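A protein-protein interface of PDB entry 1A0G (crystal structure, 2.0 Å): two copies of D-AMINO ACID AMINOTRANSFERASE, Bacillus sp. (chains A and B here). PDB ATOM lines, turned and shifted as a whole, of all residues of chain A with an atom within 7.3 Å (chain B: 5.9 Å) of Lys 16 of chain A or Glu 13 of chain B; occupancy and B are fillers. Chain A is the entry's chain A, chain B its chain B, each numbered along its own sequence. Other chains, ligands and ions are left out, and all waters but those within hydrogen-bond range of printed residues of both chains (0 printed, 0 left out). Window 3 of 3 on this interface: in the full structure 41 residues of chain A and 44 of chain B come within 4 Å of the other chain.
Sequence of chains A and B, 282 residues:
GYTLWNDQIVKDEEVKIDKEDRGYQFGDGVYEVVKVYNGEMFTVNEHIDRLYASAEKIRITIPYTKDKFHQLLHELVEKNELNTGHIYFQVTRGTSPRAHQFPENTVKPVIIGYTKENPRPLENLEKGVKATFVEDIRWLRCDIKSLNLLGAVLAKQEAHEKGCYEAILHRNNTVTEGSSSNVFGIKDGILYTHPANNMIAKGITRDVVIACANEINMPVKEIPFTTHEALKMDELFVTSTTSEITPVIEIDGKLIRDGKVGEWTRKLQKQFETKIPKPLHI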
ATOM      1  N   TRP A   5      23.504 -20.566  -6.859  1.00  0.00           N
ATOM      2  CA  TRP A   5      22.825 -19.455  -6.238  1.00  0.00           C
ATOM      3  C   TRP A   5      22.433 -19.953  -4.863  1.00  0.00           C
ATOM      4  O   TRP A   5      21.426 -20.649  -4.712  1.00  0.00           O
ATOM      5  CB  TRP A   5      21.590 -19.091  -7.056  1.00  0.00           C
ATOM      6  CG  TRP A   5      20.889 -17.869  -6.571  1.00  0.00           C
ATOM      7  CD1 TRP A   5      21.335 -16.974  -5.632  1.00  0.00           C
ATOM      8  CD2 TRP A   5      19.620 -17.378  -7.021  1.00  0.00           C
ATOM      9  NE1 TRP A   5      20.426 -15.959  -5.482  1.00  0.00           N
ATOM     10  CE2 TRP A   5      19.365 -16.179  -6.317  1.00  0.00           C
ATOM     11  CE3 TRP A   5      18.675 -17.833  -7.953  1.00  0.00           C
ATOM     12  CZ2 TRP A   5      18.204 -15.431  -6.514  1.00  0.00           C
ATOM     13  CZ3 TRP A   5      17.520 -17.090  -8.147  1.00  0.00           C
ATOM     14  CH2 TRP A   5      17.294 -15.898  -7.431  1.00  0.00           C
ATOM     15  N   VAL A  10      21.109 -23.523 -10.291  1.00  0.00           N
ATOM     16  CA  VAL A  10      20.021 -23.054 -11.134  1.00  0.00           C
ATOM     17  C   VAL A  10      20.531 -22.616 -12.498  1.00  0.00           C
ATOM     18  O   VAL A  10      21.721 -22.404 -12.666  1.00  0.00           O
ATOM     19  CB  VAL A  10      19.275 -21.863 -10.438  1.00  0.00           C
ATOM     20  CG1 VAL A  10      18.905 -22.227  -9.024  1.00  0.00           C
ATOM     21  CG2 VAL A  10      20.133 -20.615 -10.433  1.00  0.00           C
ATOM     22  N   ASP A  12      21.394 -20.164 -15.429  1.00  0.00           N
ATOM     23  CA  ASP A  12      21.832 -18.768 -15.406  1.00  0.00           C
ATOM     24  C   ASP A  12      20.699 -17.758 -15.428  1.00  0.00           C
ATOM     25  O   ASP A  12      20.690 -16.805 -14.663  1.00  0.00           O
ATOM     26  CB  ASP A  12      22.733 -18.465 -16.610  1.00  0.00           C
ATOM     27  CG  ASP A  12      24.050 -19.214 -16.574  1.00  0.00           C
ATOM     28  OD1 ASP A  12      24.418 -19.771 -15.519  1.00  0.00           O
ATOM     29  OD2 ASP A  12      24.731 -19.243 -17.621  1.00  0.00           O
ATOM     30  N   GLU A  13      19.762 -17.980 -16.341  1.00  0.00           N
ATOM     31  CA  GLU A  13      18.616 -17.107 -16.567  1.00  0.00           C
ATOM     32  C   GLU A  13      17.757 -16.819 -15.350  1.00  0.00           C
ATOM     33  O   GLU A  13      17.098 -15.787 -15.292  1.00  0.00           O
ATOM     34  CB  GLU A  13      17.708 -17.706 -17.650  1.00  0.00           C
ATOM     35  CG  GLU A  13      18.360 -17.912 -19.011  1.00  0.00           C
ATOM     36  CD  GLU A  13      19.253 -19.150 -19.078  1.00  0.00           C
ATOM     37  OE1 GLU A  13      18.939 -20.164 -18.408  1.00  0.00           O
ATOM     38  OE2 GLU A  13      20.267 -19.107 -19.812  1.00  0.00           O
ATOM     39  N   GLU A  14      17.734 -17.741 -14.399  1.00  0.00           N
ATOM     40  CA  GLU A  14      16.913 -17.569 -13.214  1.00  0.00           C
ATOM     41  C   GLU A  14      17.524 -16.732 -12.092  1.00  0.00           C
ATOM     42  O   GLU A  14      16.809 -16.312 -11.180  1.00  0.00           O
ATOM     43  CB  GLU A  14      16.496 -18.935 -12.668  1.00  0.00           C
ATOM     44  CG  GLU A  14      15.650 -19.780 -13.625  1.00  0.00           C
ATOM     45  CD  GLU A  14      14.906 -20.904 -12.911  1.00  0.00           C
ATOM     46  OE1 GLU A  14      15.525 -21.952 -12.606  1.00  0.00           O
ATOM     47  OE2 GLU A  14      13.693 -20.736 -12.643  1.00  0.00           O
ATOM     48  N   VAL A  15      18.831 -16.481 -12.157  1.00  0.00           N
ATOM     49  CA  VAL A  15      19.511 -15.725 -11.108  1.00  0.00           C
ATOM     50  C   VAL A  15      19.204 -14.233 -11.164  1.00  0.00           C
ATOM     51  O   VAL A  15      19.311 -13.594 -12.216  1.00  0.00           O
ATOM     52  CB  VAL A  15      21.054 -15.958 -11.131  1.00  0.00           C
ATOM     53  CG1 VAL A  15      21.714 -15.216  -9.972  1.00  0.00           C
ATOM     54  CG2 VAL A  15      21.366 -17.432 -11.026  1.00  0.00           C
ATOM     55  N   LYS A  16      18.781 -13.685 -10.033  1.00  0.00           N
ATOM     56  CA  LYS A  16      18.477 -12.261  -9.969  1.00  0.00           C
ATOM     57  C   LYS A  16      19.149 -11.621  -8.768  1.00  0.00           C
ATOM     58  O   LYS A  16      19.022 -12.104  -7.645  1.00  0.00           O
ATOM     59  CB  LYS A  16      16.961 -12.018  -9.913  1.00  0.00           C
ATOM     60  CG  LYS A  16      16.258 -12.040 -11.283  1.00  0.00           C
ATOM     61  CD  LYS A  16      14.772 -11.681 -11.149  1.00  0.00           C
ATOM     62  CE  LYS A  16      14.567 -10.420 -10.268  1.00  0.00           C
ATOM     63  NZ  LYS A  16      13.115 -10.237  -9.859  1.00  0.00           N
ATOM     64  N   ILE A  17      19.860 -10.525  -9.021  1.00  0.00           N
ATOM     65  CA  ILE A  17      20.557  -9.796  -7.975  1.00  0.00           C
ATOM     66  C   ILE A  17      19.668  -8.629  -7.547  1.00  0.00           C
ATOM     67  O   ILE A  17      19.215  -7.847  -8.380  1.00  0.00           O
ATOM     68  CB  ILE A  17      21.910  -9.243  -8.486  1.00  0.00           C
ATOM     69  CG1 ILE A  17      22.781 -10.373  -9.052  1.00  0.00           C
ATOM     70  CG2 ILE A  17      22.624  -8.456  -7.400  1.00  0.00           C
ATOM     71  CD1 ILE A  17      22.955 -11.567  -8.144  1.00  0.00           C
ATOM     72  N   ASP A  18      19.418  -8.527  -6.252  1.00  0.00           N
ATOM     73  CA  ASP A  18      18.588  -7.464  -5.695  1.00  0.00           C
ATOM     74  C   ASP A  18      19.359  -6.154  -5.709  1.00  0.00           C
ATOM     75  O   ASP A  18      20.542  -6.138  -5.396  1.00  0.00           O
ATOM     76  CB  ASP A  18      18.213  -7.829  -4.265  1.00  0.00           C
ATOM     77  CG  ASP A  18      17.068  -6.995  -3.733  1.00  0.00           C
ATOM     78  OD1 ASP A  18      17.271  -5.803  -3.434  1.00  0.00           O
ATOM     79  OD2 ASP A  18      15.955  -7.540  -3.615  1.00  0.00           O
ATOM     80  N   LYS A  19      18.697  -5.049  -6.047  1.00  0.00           N
ATOM     81  CA  LYS A  19      19.362  -3.749  -6.070  1.00  0.00           C
ATOM     82  C   LYS A  19      19.985  -3.370  -4.724  1.00  0.00           C
ATOM     83  O   LYS A  19      20.903  -2.569  -4.674  1.00  0.00           O
ATOM     84  CB  LYS A  19      18.411  -2.628  -6.541  1.00  0.00           C
ATOM     85  CG  LYS A  19      17.179  -2.395  -5.651  1.00  0.00           C
ATOM     86  CD  LYS A  19      16.437  -1.092  -6.022  1.00  0.00           C
ATOM     87  CE  LYS A  19      14.944  -1.120  -5.676  1.00  0.00           C
ATOM     88  NZ  LYS A  19      14.598  -1.814  -4.408  1.00  0.00           N
ATOM     89  N   ASP A  21      21.507  -5.518  -2.607  1.00  0.00           N
ATOM     90  CA  ASP A  21      22.436  -6.538  -2.144  1.00  0.00           C
ATOM     91  C   ASP A  21      23.637  -5.668  -1.741  1.00  0.00           C
ATOM     92  O   ASP A  21      24.087  -4.824  -2.517  1.00  0.00           O
ATOM     93  CB  ASP A  21      22.825  -7.463  -3.297  1.00  0.00           C
ATOM     94  CG  ASP A  21      23.676  -8.649  -2.851  1.00  0.00           C
ATOM     95  OD1 ASP A  21      24.654  -8.470  -2.081  1.00  0.00           O
ATOM     96  OD2 ASP A  21      23.381  -9.774  -3.310  1.00  0.00           O
ATOM     97  N   VAL A 110      24.487 -13.829   0.413  1.00  0.00           N
ATOM     98  CA  VAL A 110      24.088 -14.273  -0.935  1.00  0.00           C
ATOM     99  C   VAL A 110      25.340 -14.842  -1.616  1.00  0.00           C
ATOM    100  O   VAL A 110      26.392 -14.207  -1.634  1.00  0.00           O
ATOM    101  CB  VAL A 110      23.489 -13.125  -1.775  1.00  0.00           C
ATOM    102  CG1 VAL A 110      23.180 -13.616  -3.187  1.00  0.00           C
ATOM    103  CG2 VAL A 110      22.220 -12.607  -1.102  1.00  0.00           C
ATOM    104  N   ILE A 112      27.080 -16.558  -4.973  1.00  0.00           N
ATOM    105  CA  ILE A 112      27.024 -16.682  -6.408  1.00  0.00           C
ATOM    106  C   ILE A 112      28.288 -17.368  -6.890  1.00  0.00           C
ATOM    107  O   ILE A 112      29.403 -17.023  -6.469  1.00  0.00           O
ATOM    108  CB  ILE A 112      26.936 -15.307  -7.093  1.00  0.00           C
ATOM    109  CG1 ILE A 112      25.543 -14.696  -6.892  1.00  0.00           C
ATOM    110  CG2 ILE A 112      27.234 -15.421  -8.588  1.00  0.00           C
ATOM    111  CD1 ILE A 112      24.459 -15.446  -7.599  1.00  0.00           C
ATOM    112  N   GLY B   1       7.511   0.004  -4.518  1.00  0.00           N
ATOM    113  CA  GLY B   1       7.270   1.299  -5.178  1.00  0.00           C
ATOM    114  C   GLY B   1       7.787   1.242  -6.602  1.00  0.00           C
ATOM    115  O   GLY B   1       7.657   0.220  -7.277  1.00  0.00           O
ATOM    116  N   LYS B  11       8.211  -0.575 -12.083  1.00  0.00           N
ATOM    117  CA  LYS B  11       7.863  -1.127 -10.777  1.00  0.00           C
ATOM    118  C   LYS B  11       9.077  -1.904 -10.272  1.00  0.00           C
ATOM    119  O   LYS B  11       9.761  -2.539 -11.076  1.00  0.00           O
ATOM    120  CB  LYS B  11       6.636  -2.032 -10.897  1.00  0.00           C
ATOM    121  CG  LYS B  11       5.348  -1.259 -11.147  1.00  0.00           C
ATOM    122  CD  LYS B  11       4.142  -2.163 -11.433  1.00  0.00           C
ATOM    123  CE  LYS B  11       3.838  -3.108 -10.265  1.00  0.00           C
ATOM    124  NZ  LYS B  11       2.721  -4.074 -10.533  1.00  0.00           N
ATOM    125  N   ASP B  12       9.339  -1.883  -8.969  1.00  0.00           N
ATOM    126  CA  ASP B  12      10.512  -2.574  -8.414  1.00  0.00           C
ATOM    127  C   ASP B  12      10.747  -4.005  -8.881  1.00  0.00           C
ATOM    128  O   ASP B  12      11.887  -4.436  -9.048  1.00  0.00           O
ATOM    129  CB  ASP B  12      10.460  -2.588  -6.884  1.00  0.00           C
ATOM    130  CG  ASP B  12      10.461  -1.199  -6.277  1.00  0.00           C
ATOM    131  OD1 ASP B  12      10.813  -0.225  -6.974  1.00  0.00           O
ATOM    132  OD2 ASP B  12      10.106  -1.079  -5.080  1.00  0.00           O
ATOM    133  N   GLU B  13       9.668  -4.741  -9.072  1.00  0.00           N
ATOM    134  CA  GLU B  13       9.709  -6.144  -9.478  1.00  0.00           C
ATOM    135  C   GLU B  13      10.283  -6.405 -10.869  1.00  0.00           C
ATOM    136  O   GLU B  13      10.633  -7.540 -11.187  1.00  0.00           O
ATOM    137  CB  GLU B  13       8.294  -6.725  -9.424  1.00  0.00           C
ATOM    138  CG  GLU B  13       7.466  -6.247  -8.251  1.00  0.00           C
ATOM    139  CD  GLU B  13       6.397  -5.235  -8.648  1.00  0.00           C
ATOM    140  OE1 GLU B  13       5.468  -5.625  -9.399  1.00  0.00           O
ATOM    141  OE2 GLU B  13       6.490  -4.057  -8.210  1.00  0.00           O
ATOM    142  N   GLU B  14      10.298  -5.398 -11.717  1.00  0.00           N
ATOM    143  CA  GLU B  14      10.771  -5.570 -13.065  1.00  0.00           C
ATOM    144  C   GLU B  14      12.276  -5.471 -13.187  1.00  0.00           C
ATOM    145  O   GLU B  14      12.862  -5.914 -14.178  1.00  0.00           O
ATOM    146  CB  GLU B  14      10.112  -4.518 -13.947  1.00  0.00           C
ATOM    147  CG  GLU B  14       8.622  -4.768 -14.225  1.00  0.00           C
ATOM    148  CD  GLU B  14       7.965  -3.632 -14.987  1.00  0.00           C
ATOM    149  OE1 GLU B  14       8.343  -3.375 -16.155  1.00  0.00           O
ATOM    150  OE2 GLU B  14       7.060  -2.982 -14.411  1.00  0.00           O
ATOM    151  N   VAL B  15      12.895  -4.834 -12.198  1.00  0.00           N
ATOM    152  CA  VAL B  15      14.336  -4.617 -12.192  1.00  0.00           C
ATOM    153  C   VAL B  15      15.077  -5.933 -11.995  1.00  0.00           C
ATOM    154  O   VAL B  15      14.733  -6.728 -11.116  1.00  0.00           O
ATOM    155  CB  VAL B  15      14.759  -3.634 -11.058  1.00  0.00           C
ATOM    156  CG1 VAL B  15      16.245  -3.292 -11.171  1.00  0.00           C
ATOM    157  CG2 VAL B  15      13.919  -2.359 -11.108  1.00  0.00           C
ATOM    158  N   LYS B  16      16.077  -6.166 -12.837  1.00  0.00           N
ATOM    159  CA  LYS B  16      16.900  -7.360 -12.748  1.00  0.00           C
ATOM    160  C   LYS B  16      18.373  -6.974 -12.871  1.00  0.00           C
ATOM    161  O   LYS B  16      18.788  -6.326 -13.834  1.00  0.00           O
ATOM    162  CB  LYS B  16      16.521  -8.368 -13.840  1.00  0.00           C
ATOM    163  CG  LYS B  16      15.197  -9.103 -13.557  1.00  0.00           C
ATOM    164  CD  LYS B  16      14.902 -10.215 -14.575  1.00  0.00           C
ATOM    165  CE  LYS B  16      14.472  -9.663 -15.935  1.00  0.00           C
ATOM    166  NZ  LYS B  16      14.141 -10.809 -16.847  1.00  0.00           N
ATOM    167  N   ILE B  17      19.153  -7.295 -11.851  1.00  0.00           N
ATOM    168  CA  ILE B  17      20.572  -6.990 -11.899  1.00  0.00           C
ATOM    169  C   ILE B  17      21.281  -8.276 -12.267  1.00  0.00           C
ATOM    170  O   ILE B  17      20.981  -9.342 -11.729  1.00  0.00           O
ATOM    171  CB  ILE B  17      21.111  -6.504 -10.545  1.00  0.00           C
ATOM    172  CG1 ILE B  17      20.180  -5.440  -9.931  1.00  0.00           C
ATOM    173  CG2 ILE B  17      22.537  -5.995 -10.719  1.00  0.00           C
ATOM    174  CD1 ILE B  17      20.042  -4.179 -10.720  1.00  0.00           C
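The backbone carbonyl oxygen (O) of Ile 17 of chain B lies within hydrogen-bond range of the backbone NH (N) of Ile 17 of chain A, at 3.2 Å.
NZ of Lys 11 of chain B lies within salt-bridge range of OE1 of Glu 13 of chain B, 3.4 Å away.
Among the printed residues, merely in contact across the chains: Lys 16 of chain A with Lys 16 of chain B (3.6 Å), Lys 16 of chain A with Val 15 of chain B (3.8 Å) and Lys 16 of chain A with Glu 13 of chain B (3.9 Å).
Of the printed residues of chain B, Ile 17 of chain A touches Ile 17.
Of the printed residues of chain A, Glu 13 of chain B touches Lys 16 (3.9 Å).
Of the printed residues of chain A, Val 15 of chain B touches Lys 16 (3.8 Å).
Printed residues of chain A within 4 Å of Lys 16 of chain B: Lys 16 (3.6 Å).
Printed residues of chain A within 4 Å of Ile 17 of chain B: Ile 17.
The nearest residue of chain A that does not touch Glu 13 of chain B is Lys 19 of chain A (7.2 Å).
The nearest printed residue of chain A that does not touch Val 15 of chain B is Lys 19 of chain A (5.2 Å).
Of the 13 printed residues of chain A, 2 touch a printed residue of chain B.
Of the 8 printed residues of chain B, 4 touch a printed residue of chain A.
Lys 16 of chain A touches Glu 13 of chain B, but with the chains exchanged Glu 13 of chain A does not touch Lys 16 of chain B (6.0 Å).
Lys 16 of chain A touches Val 15 of chain B, but with the chains exchanged Val 15 of chain A does not touch Lys 16 of chain B (6.0 Å).
Lys 16 of chain A touches its own counterpart, Lys 16 of chain B.
Ile 17 of chain B touches its own counterpart, Ile 17 of chain A.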
